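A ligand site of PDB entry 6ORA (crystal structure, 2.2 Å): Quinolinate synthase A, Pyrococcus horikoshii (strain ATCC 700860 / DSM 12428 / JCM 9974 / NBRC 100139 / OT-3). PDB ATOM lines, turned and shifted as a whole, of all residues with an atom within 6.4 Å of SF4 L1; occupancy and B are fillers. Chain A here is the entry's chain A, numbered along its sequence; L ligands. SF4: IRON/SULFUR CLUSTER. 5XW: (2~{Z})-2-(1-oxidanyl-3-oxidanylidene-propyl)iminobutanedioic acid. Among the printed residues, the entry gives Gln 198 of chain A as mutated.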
ATOM      1  N   HIS A  21      -7.555   7.545   7.438  1.00  0.00           N
ATOM      2  CA  HIS A  21      -7.823   8.651   6.525  1.00  0.00           C
ATOM      3  C   HIS A  21      -9.265   9.108   6.676  1.00  0.00           C
ATOM      4  O   HIS A  21     -10.128   8.375   7.171  1.00  0.00           O
ATOM      5  CB  HIS A  21      -7.533   8.242   5.080  1.00  0.00           C
ATOM      6  CG  HIS A  21      -7.667   9.352   4.098  1.00  0.00           C
ATOM      7  ND1 HIS A  21      -8.749   9.457   3.232  1.00  0.00           N
ATOM      8  CD2 HIS A  21      -6.883  10.420   3.844  1.00  0.00           C
ATOM      9  CE1 HIS A  21      -8.606  10.541   2.489  1.00  0.00           C
ATOM     10  NE2 HIS A  21      -7.486  11.143   2.839  1.00  0.00           N
ATOM     11  N   TYR A  23     -11.492   9.307   4.595  1.00  0.00           N
ATOM     12  CA  TYR A  23     -12.418   8.514   3.810  1.00  0.00           C
ATOM     13  C   TYR A  23     -12.755   7.176   4.454  1.00  0.00           C
ATOM     14  O   TYR A  23     -13.456   6.367   3.830  1.00  0.00           O
ATOM     15  CB  TYR A  23     -11.864   8.272   2.399  1.00  0.00           C
ATOM     16  CG  TYR A  23     -11.680   9.524   1.558  1.00  0.00           C
ATOM     17  CD1 TYR A  23     -12.231  10.741   1.948  1.00  0.00           C
ATOM     18  CD2 TYR A  23     -10.963   9.473   0.369  1.00  0.00           C
ATOM     19  CE1 TYR A  23     -12.064  11.880   1.175  1.00  0.00           C
ATOM     20  CE2 TYR A  23     -10.789  10.603  -0.411  1.00  0.00           C
ATOM     21  CZ  TYR A  23     -11.340  11.799  -0.002  1.00  0.00           C
ATOM     22  OH  TYR A  23     -11.174  12.937  -0.774  1.00  0.00           O
ATOM     23  N   VAL A  58      -5.309   3.305   2.280  1.00  0.00           N
ATOM     24  CA  VAL A  58      -4.906   2.586   1.076  1.00  0.00           C
ATOM     25  C   VAL A  58      -3.403   2.295   1.102  1.00  0.00           C
ATOM     26  O   VAL A  58      -2.680   2.802   1.975  1.00  0.00           O
ATOM     27  CB  VAL A  58      -5.295   3.362  -0.193  1.00  0.00           C
ATOM     28  CG1 VAL A  58      -6.784   3.171  -0.472  1.00  0.00           C
ATOM     29  CG2 VAL A  58      -4.972   4.840  -0.028  1.00  0.00           C
ATOM     30  N   PHE A  60      -0.703   3.007  -0.773  1.00  0.00           N
ATOM     31  CA  PHE A  60       0.337   4.034  -0.907  1.00  0.00           C
ATOM     32  C   PHE A  60       0.469   4.842   0.368  1.00  0.00           C
ATOM     33  O   PHE A  60       1.559   5.364   0.661  1.00  0.00           O
ATOM     34  CB  PHE A  60       0.055   4.928  -2.121  1.00  0.00           C
ATOM     35  CG  PHE A  60      -0.977   6.015  -1.892  1.00  0.00           C
ATOM     36  CD1 PHE A  60      -0.637   7.200  -1.250  1.00  0.00           C
ATOM     37  CD2 PHE A  60      -2.271   5.871  -2.354  1.00  0.00           C
ATOM     38  CE1 PHE A  60      -1.572   8.201  -1.038  1.00  0.00           C
ATOM     39  CE2 PHE A  60      -3.220   6.874  -2.168  1.00  0.00           C
ATOM     40  CZ  PHE A  60      -2.871   8.029  -1.500  1.00  0.00           C
ATOM     41  N   MET A  61      -0.614   4.979   1.134  1.00  0.00           N
ATOM     42  CA  MET A  61      -0.526   5.693   2.412  1.00  0.00           C
ATOM     43  C   MET A  61       0.262   4.892   3.437  1.00  0.00           C
ATOM     44  O   MET A  61       1.086   5.458   4.169  1.00  0.00           O
ATOM     45  CB  MET A  61      -1.937   6.000   2.930  1.00  0.00           C
ATOM     46  CG  MET A  61      -2.700   7.036   2.126  1.00  0.00           C
ATOM     47  SD  MET A  61      -4.357   7.341   2.772  1.00  0.00           S
ATOM     48  CE  MET A  61      -4.933   8.585   1.637  1.00  0.00           C
ATOM     49  N   THR A  82      -6.384  -0.361  -2.153  1.00  0.00           N
ATOM     50  CA  THR A  82      -5.476   0.283  -3.080  1.00  0.00           C
ATOM     51  C   THR A  82      -6.138   1.520  -3.681  1.00  0.00           C
ATOM     52  O   THR A  82      -7.346   1.728  -3.560  1.00  0.00           O
ATOM     53  CB  THR A  82      -5.025  -0.680  -4.194  1.00  0.00           C
ATOM     54  OG1 THR A  82      -4.019  -0.054  -4.993  1.00  0.00           O
ATOM     55  CG2 THR A  82      -6.210  -1.053  -5.074  1.00  0.00           C
ATOM     56  N   CYS A  83      -5.318   2.336  -4.338  1.00  0.00           N
ATOM     57  CA  CYS A  83      -5.743   3.587  -4.937  1.00  0.00           C
ATOM     58  C   CYS A  83      -5.721   3.442  -6.455  1.00  0.00           C
ATOM     59  O   CYS A  83      -4.645   3.215  -7.037  1.00  0.00           O
ATOM     60  CB  CYS A  83      -4.854   4.744  -4.494  1.00  0.00           C
ATOM     61  SG  CYS A  83      -5.070   6.280  -5.417  1.00  0.00           S
ATOM     62  N   ALA A  84      -6.885   3.589  -7.086  1.00  0.00           N
ATOM     63  CA  ALA A  84      -6.973   3.387  -8.533  1.00  0.00           C
ATOM     64  C   ALA A  84      -6.155   4.434  -9.294  1.00  0.00           C
ATOM     65  O   ALA A  84      -5.513   4.104 -10.299  1.00  0.00           O
ATOM     66  CB  ALA A  84      -8.432   3.424  -8.978  1.00  0.00           C
ATOM     67  N   MET A  85      -6.169   5.684  -8.835  1.00  0.00           N
ATOM     68  CA  MET A  85      -5.445   6.736  -9.546  1.00  0.00           C
ATOM     69  C   MET A  85      -3.945   6.544  -9.429  1.00  0.00           C
ATOM     70  O   MET A  85      -3.209   6.750 -10.402  1.00  0.00           O
ATOM     71  CB  MET A  85      -5.860   8.109  -9.019  1.00  0.00           C
ATOM     72  CG  MET A  85      -5.156   9.272  -9.701  1.00  0.00           C
ATOM     73  SD  MET A  85      -3.853   9.966  -8.680  1.00  0.00           S
ATOM     74  CE  MET A  85      -4.824  10.515  -7.282  1.00  0.00           C
ATOM     75  N   ALA A  86      -3.464   6.128  -8.243  1.00  0.00           N
ATOM     76  CA  ALA A  86      -2.032   5.943  -8.044  1.00  0.00           C
ATOM     77  C   ALA A  86      -1.457   4.907  -9.001  1.00  0.00           C
ATOM     78  O   ALA A  86      -0.376   5.116  -9.571  1.00  0.00           O
ATOM     79  CB  ALA A  86      -1.760   5.517  -6.594  1.00  0.00           C
ATOM     80  N   TYR A 109       2.374  13.211  -7.074  1.00  0.00           N
ATOM     81  CA  TYR A 109       1.349  13.061  -6.044  1.00  0.00           C
ATOM     82  C   TYR A 109       1.730  11.930  -5.098  1.00  0.00           C
ATOM     83  O   TYR A 109       2.285  10.905  -5.515  1.00  0.00           O
ATOM     84  CB  TYR A 109       0.010  12.757  -6.721  1.00  0.00           C
ATOM     85  CG  TYR A 109      -1.243  13.309  -6.071  1.00  0.00           C
ATOM     86  CD1 TYR A 109      -1.198  14.002  -4.859  1.00  0.00           C
ATOM     87  CD2 TYR A 109      -2.488  13.146  -6.668  1.00  0.00           C
ATOM     88  CE1 TYR A 109      -2.346  14.497  -4.269  1.00  0.00           C
ATOM     89  CE2 TYR A 109      -3.640  13.634  -6.099  1.00  0.00           C
ATOM     90  CZ  TYR A 109      -3.568  14.317  -4.899  1.00  0.00           C
ATOM     91  OH  TYR A 109      -4.730  14.807  -4.328  1.00  0.00           O
ATOM     92  N   ASN A 111      -0.231   9.942  -3.877  1.00  0.00           N
ATOM     93  CA  ASN A 111      -0.943   8.826  -4.478  1.00  0.00           C
ATOM     94  C   ASN A 111      -0.098   8.283  -5.622  1.00  0.00           C
ATOM     95  O   ASN A 111      -0.295   8.606  -6.802  1.00  0.00           O
ATOM     96  CB  ASN A 111      -2.322   9.253  -4.974  1.00  0.00           C
ATOM     97  CG  ASN A 111      -3.060  10.120  -3.981  1.00  0.00           C
ATOM     98  OD1 ASN A 111      -2.470  11.010  -3.358  1.00  0.00           O
ATOM     99  ND2 ASN A 111      -4.351   9.860  -3.819  1.00  0.00           N
ATOM    100  N   ASP A 146      -2.331  12.510 -11.229  1.00  0.00           N
ATOM    101  CA  ASP A 146      -3.691  12.997 -11.381  1.00  0.00           C
ATOM    102  C   ASP A 146      -3.730  14.213 -12.307  1.00  0.00           C
ATOM    103  O   ASP A 146      -3.170  15.272 -11.987  1.00  0.00           O
ATOM    104  CB  ASP A 146      -4.278  13.346 -10.018  1.00  0.00           C
ATOM    105  CG  ASP A 146      -5.753  13.663 -10.090  1.00  0.00           C
ATOM    106  OD1 ASP A 146      -6.103  14.777 -10.527  1.00  0.00           O
ATOM    107  OD2 ASP A 146      -6.566  12.782  -9.738  1.00  0.00           O
ATOM    108  N   HIS A 169      -6.274   9.942 -13.330  1.00  0.00           N
ATOM    109  CA  HIS A 169      -7.415  10.578 -12.692  1.00  0.00           C
ATOM    110  C   HIS A 169      -7.956   9.646 -11.615  1.00  0.00           C
ATOM    111  O   HIS A 169      -7.644   8.454 -11.569  1.00  0.00           O
ATOM    112  CB  HIS A 169      -8.506  10.902 -13.704  1.00  0.00           C
ATOM    113  CG  HIS A 169      -9.203   9.690 -14.247  1.00  0.00           C
ATOM    114  ND1 HIS A 169      -8.742   8.989 -15.344  1.00  0.00           N
ATOM    115  CD2 HIS A 169     -10.320   9.040 -13.827  1.00  0.00           C
ATOM    116  CE1 HIS A 169      -9.549   7.972 -15.577  1.00  0.00           C
ATOM    117  NE2 HIS A 169     -10.509   7.980 -14.685  1.00  0.00           N
ATOM    118  N   CYS A 170      -8.811  10.205 -10.762  1.00  0.00           N
ATOM    119  CA  CYS A 170      -9.505   9.455  -9.727  1.00  0.00           C
ATOM    120  C   CYS A 170     -10.985   9.357 -10.111  1.00  0.00           C
ATOM    121  O   CYS A 170     -11.645  10.391 -10.286  1.00  0.00           O
ATOM    122  CB  CYS A 170      -9.348  10.128  -8.361  1.00  0.00           C
ATOM    123  SG  CYS A 170     -10.705   9.768  -7.222  1.00  0.00           S
ATOM    124  N   TYR A 171     -11.480   8.126 -10.233  1.00  0.00           N
ATOM    125  CA  TYR A 171     -12.845   7.921 -10.701  1.00  0.00           C
ATOM    126  C   TYR A 171     -13.869   8.422  -9.692  1.00  0.00           C
ATOM    127  O   TYR A 171     -14.969   8.826 -10.077  1.00  0.00           O
ATOM    128  CB  TYR A 171     -13.076   6.446 -11.007  1.00  0.00           C
ATOM    129  CG  TYR A 171     -13.178   5.567  -9.782  1.00  0.00           C
ATOM    130  CD1 TYR A 171     -12.041   5.137  -9.117  1.00  0.00           C
ATOM    131  CD2 TYR A 171     -14.414   5.155  -9.299  1.00  0.00           C
ATOM    132  CE1 TYR A 171     -12.130   4.322  -7.998  1.00  0.00           C
ATOM    133  CE2 TYR A 171     -14.512   4.349  -8.185  1.00  0.00           C
ATOM    134  CZ  TYR A 171     -13.365   3.931  -7.536  1.00  0.00           C
ATOM    135  OH  TYR A 171     -13.463   3.133  -6.429  1.00  0.00           O
ATOM    136  N   VAL A 172     -13.530   8.397  -8.397  1.00  0.00           N
ATOM    137  CA  VAL A 172     -14.466   8.857  -7.373  1.00  0.00           C
ATOM    138  C   VAL A 172     -14.765  10.344  -7.557  1.00  0.00           C
ATOM    139  O   VAL A 172     -15.926  10.776  -7.547  1.00  0.00           O
ATOM    140  CB  VAL A 172     -13.904   8.574  -5.971  1.00  0.00           C
ATOM    141  CG1 VAL A 172     -14.802   9.176  -4.896  1.00  0.00           C
ATOM    142  CG2 VAL A 172     -13.737   7.070  -5.762  1.00  0.00           C
ATOM    143  N   HIS A 173     -13.721  11.157  -7.731  1.00  0.00           N
ATOM    144  CA  HIS A 173     -13.911  12.583  -7.876  1.00  0.00           C
ATOM    145  C   HIS A 173     -14.374  12.980  -9.272  1.00  0.00           C
ATOM    146  O   HIS A 173     -14.975  14.047  -9.426  1.00  0.00           O
ATOM    147  CB  HIS A 173     -12.617  13.324  -7.523  1.00  0.00           C
ATOM    148  CG  HIS A 173     -12.335  13.354  -6.053  1.00  0.00           C
ATOM    149  ND1 HIS A 173     -11.612  12.357  -5.413  1.00  0.00           N
ATOM    150  CD2 HIS A 173     -12.699  14.229  -5.090  1.00  0.00           C
ATOM    151  CE1 HIS A 173     -11.534  12.643  -4.124  1.00  0.00           C
ATOM    152  NE2 HIS A 173     -12.184  13.765  -3.897  1.00  0.00           N
ATOM    153  N   GLN A 198      -9.143  17.184  -7.134  1.00  0.00           N
ATOM    154  CA  GLN A 198      -9.178  16.053  -8.052  1.00  0.00           C
ATOM    155  C   GLN A 198     -10.422  16.032  -8.923  1.00  0.00           C
ATOM    156  O   GLN A 198     -10.535  15.162  -9.797  1.00  0.00           O
ATOM    157  CB  GLN A 198      -9.076  14.731  -7.283  1.00  0.00           C
ATOM    158  CG  GLN A 198      -7.694  14.467  -6.716  1.00  0.00           C
ATOM    159  CD  GLN A 198      -7.621  13.157  -5.950  1.00  0.00           C
ATOM    160  OE1 GLN A 198      -8.428  12.254  -6.163  1.00  0.00           O
ATOM    161  NE2 GLN A 198      -6.656  13.054  -5.053  1.00  0.00           N
ATOM    162  N   GLU A 231     -15.198  12.410  -1.571  1.00  0.00           N
ATOM    163  CA  GLU A 231     -15.641  11.080  -1.169  1.00  0.00           C
ATOM    164  C   GLU A 231     -16.646  11.160  -0.024  1.00  0.00           C
ATOM    165  O   GLU A 231     -16.583  12.053   0.829  1.00  0.00           O
ATOM    166  CB  GLU A 231     -14.441  10.217  -0.761  1.00  0.00           C
ATOM    167  CG  GLU A 231     -14.629   8.712  -0.953  1.00  0.00           C
ATOM    168  CD  GLU A 231     -15.244   8.038   0.267  1.00  0.00           C
ATOM    169  OE1 GLU A 231     -15.401   8.709   1.306  1.00  0.00           O
ATOM    170  OE2 GLU A 231     -15.546   6.827   0.184  1.00  0.00           O
ATOM    171  N   CYS A 256     -15.190   5.474  -2.300  1.00  0.00           N
ATOM    172  CA  CYS A 256     -13.973   4.823  -2.750  1.00  0.00           C
ATOM    173  C   CYS A 256     -13.962   3.372  -2.267  1.00  0.00           C
ATOM    174  O   CYS A 256     -13.906   3.105  -1.058  1.00  0.00           O
ATOM    175  CB  CYS A 256     -12.737   5.576  -2.253  1.00  0.00           C
ATOM    176  SG  CYS A 256     -11.199   4.724  -2.607  1.00  0.00           S
ATOM    177  N   ILE A 257     -14.015   2.437  -3.224  1.00  0.00           N
ATOM    178  CA  ILE A 257     -14.082   1.016  -2.886  1.00  0.00           C
ATOM    179  C   ILE A 257     -12.824   0.580  -2.152  1.00  0.00           C
ATOM    180  O   ILE A 257     -12.892  -0.170  -1.169  1.00  0.00           O
ATOM    181  CB  ILE A 257     -14.311   0.180  -4.164  1.00  0.00           C
ATOM    182  CG1 ILE A 257     -15.583   0.646  -4.879  1.00  0.00           C
ATOM    183  CG2 ILE A 257     -14.396  -1.296  -3.825  1.00  0.00           C
ATOM    184  CD1 ILE A 257     -15.830  -0.065  -6.199  1.00  0.00           C
ATOM    185  N   GLY A 258     -11.658   1.045  -2.609  1.00  0.00           N
ATOM    186  CA  GLY A 258     -10.414   0.663  -1.964  1.00  0.00           C
ATOM    187  C   GLY A 258     -10.353   1.098  -0.516  1.00  0.00           C
ATOM    188  O   GLY A 258      -9.864   0.367   0.347  1.00  0.00           O
ATOM    189  N   MET A 259     -10.858   2.305  -0.227  1.00  0.00           N
ATOM    190  CA  MET A 259     -10.870   2.795   1.148  1.00  0.00           C
ATOM    191  C   MET A 259     -11.765   1.936   2.035  1.00  0.00           C
ATOM    192  O   MET A 259     -11.446   1.695   3.201  1.00  0.00           O
ATOM    193  CB  MET A 259     -11.326   4.251   1.178  1.00  0.00           C
ATOM    194  CG  MET A 259     -10.245   5.235   0.806  1.00  0.00           C
ATOM    195  SD  MET A 259      -9.143   5.593   2.183  1.00  0.00           S
ATOM    196  CE  MET A 259      -8.025   6.753   1.401  1.00  0.00           C
HETATM  197 FE1  SF4 L   1      -9.628   8.467  -5.674  1.00  0.00          FE
HETATM  198 FE2  SF4 L   1      -8.348   8.880  -2.932  1.00  0.00          FE
HETATM  199 FE3  SF4 L   1      -7.161   6.811  -4.886  1.00  0.00          FE
HETATM  200 FE4  SF4 L   1      -9.858   6.254  -3.562  1.00  0.00          FE
HETATM  201  S1  SF4 L   1      -7.858   6.751  -2.818  1.00  0.00           S
HETATM  202  S2  SF4 L   1      -9.161   6.321  -5.636  1.00  0.00           S
HETATM  203  S3  SF4 L   1     -10.369   8.386  -3.615  1.00  0.00           S
HETATM  204  S4  SF4 L   1      -7.608   8.948  -4.991  1.00  0.00           S
HETATM  205  OAD 5XW L   2      -5.975  11.369  -2.895  1.00  0.00           O
HETATM  206  CAC 5XW L   2      -6.829  11.476  -1.998  1.00  0.00           C
HETATM  207  OAE 5XW L   2      -7.296  10.488  -1.406  1.00  0.00           O
HETATM  208  CAA 5XW L   2      -7.340  12.895  -1.612  1.00  0.00           C
HETATM  209  CAB 5XW L   2      -6.415  13.597  -0.602  1.00  0.00           C
HETATM  210  CAG 5XW L   2      -7.215  14.283   0.563  1.00  0.00           C
HETATM  211  OAI 5XW L   2      -7.262  13.699   1.665  1.00  0.00           O
HETATM  212  OAH 5XW L   2      -7.753  15.400   0.303  1.00  0.00           O
HETATM  213  NAF 5XW L   2      -5.112  13.626  -0.733  1.00  0.00           N
HETATM  214  CAJ 5XW L   2      -4.077  14.182  -0.010  1.00  0.00           C
HETATM  215  OAN 5XW L   2      -3.028  14.673  -0.806  1.00  0.00           O
HETATM  216  CAK 5XW L   2      -4.458  15.231   1.006  1.00  0.00           C
HETATM  217  CAL 5XW L   2      -3.238  15.636   1.818  1.00  0.00           C
HETATM  218  OAM 5XW L   2      -2.947  16.805   1.931  1.00  0.00           O
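An oxygen (OAE) of 5XW L2 binds an iron atom (FE2) of SF4 L1, 2.5 Å away.
FE3 of SF4 L1 is bound by SG of Cys 83, 2.2 Å away. A ring nitrogen (NE2) of His 21 is in hydrogen-bond range of an oxygen (OAI) of 5XW L2, at 2.8 Å. An iron atom (FE4) of SF4 L1 is bound by the side-chain sulfur of Cys 256 (2.2 Å). The side-chain amide oxygen (OE1) of Gln 198 sits close to a sulfur (S4) of SF4 L1 (3.6 Å). S4 of SF4 L1 lies close to ND2 of Asn 111 (3.6 Å). NE2 of Gln 198 is in hydrogen-bond range of OAD of 5XW L2 (2.8 Å). The side-chain sulfur (SG) of Cys 170 binds an iron atom (FE1) of SF4 L1 (2.3 Å). ND2 of Asn 111 lies within hydrogen-bond range of OAD of 5XW L2 (2.4 Å).
Residues that only touch SF4 L1: Ala 84 (3.8 Å), Tyr 23 (3.9 Å) and Met 85 (3.9 Å). Hydrophobic or aromatic side chains that line SF4 L1: Tyr 23 and Met 85. The nearest printed residue that does not touch SF4 L1 is Val 172 (4.2 Å).
The backbone NH of Gly 258 lies close to the side-chain sulfur of Cys 256 (3.7 Å). The side-chain hydroxyl (OH) of Tyr 23 lies close to a ring nitrogen (NE2) of His 173, at 3.4 Å. The side-chain sulfur (SG) of Cys 170 sits close to the backbone NH (N) of Val 172 (3.4 Å). N of Ala 86 lies close to SG of Cys 83 (3.3 Å). N of Cys 256 lies within hydrogen-bond range of OE2 of Glu 231 (2.9 Å). SG of Cys 170 sits close to OE1 of Gln 198, at 3.5 Å. SG of Cys 83 lies close to N of Met 85, at 3.6 Å. ND1 of His 173 sits close to SG of Cys 170 (3.3 Å).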
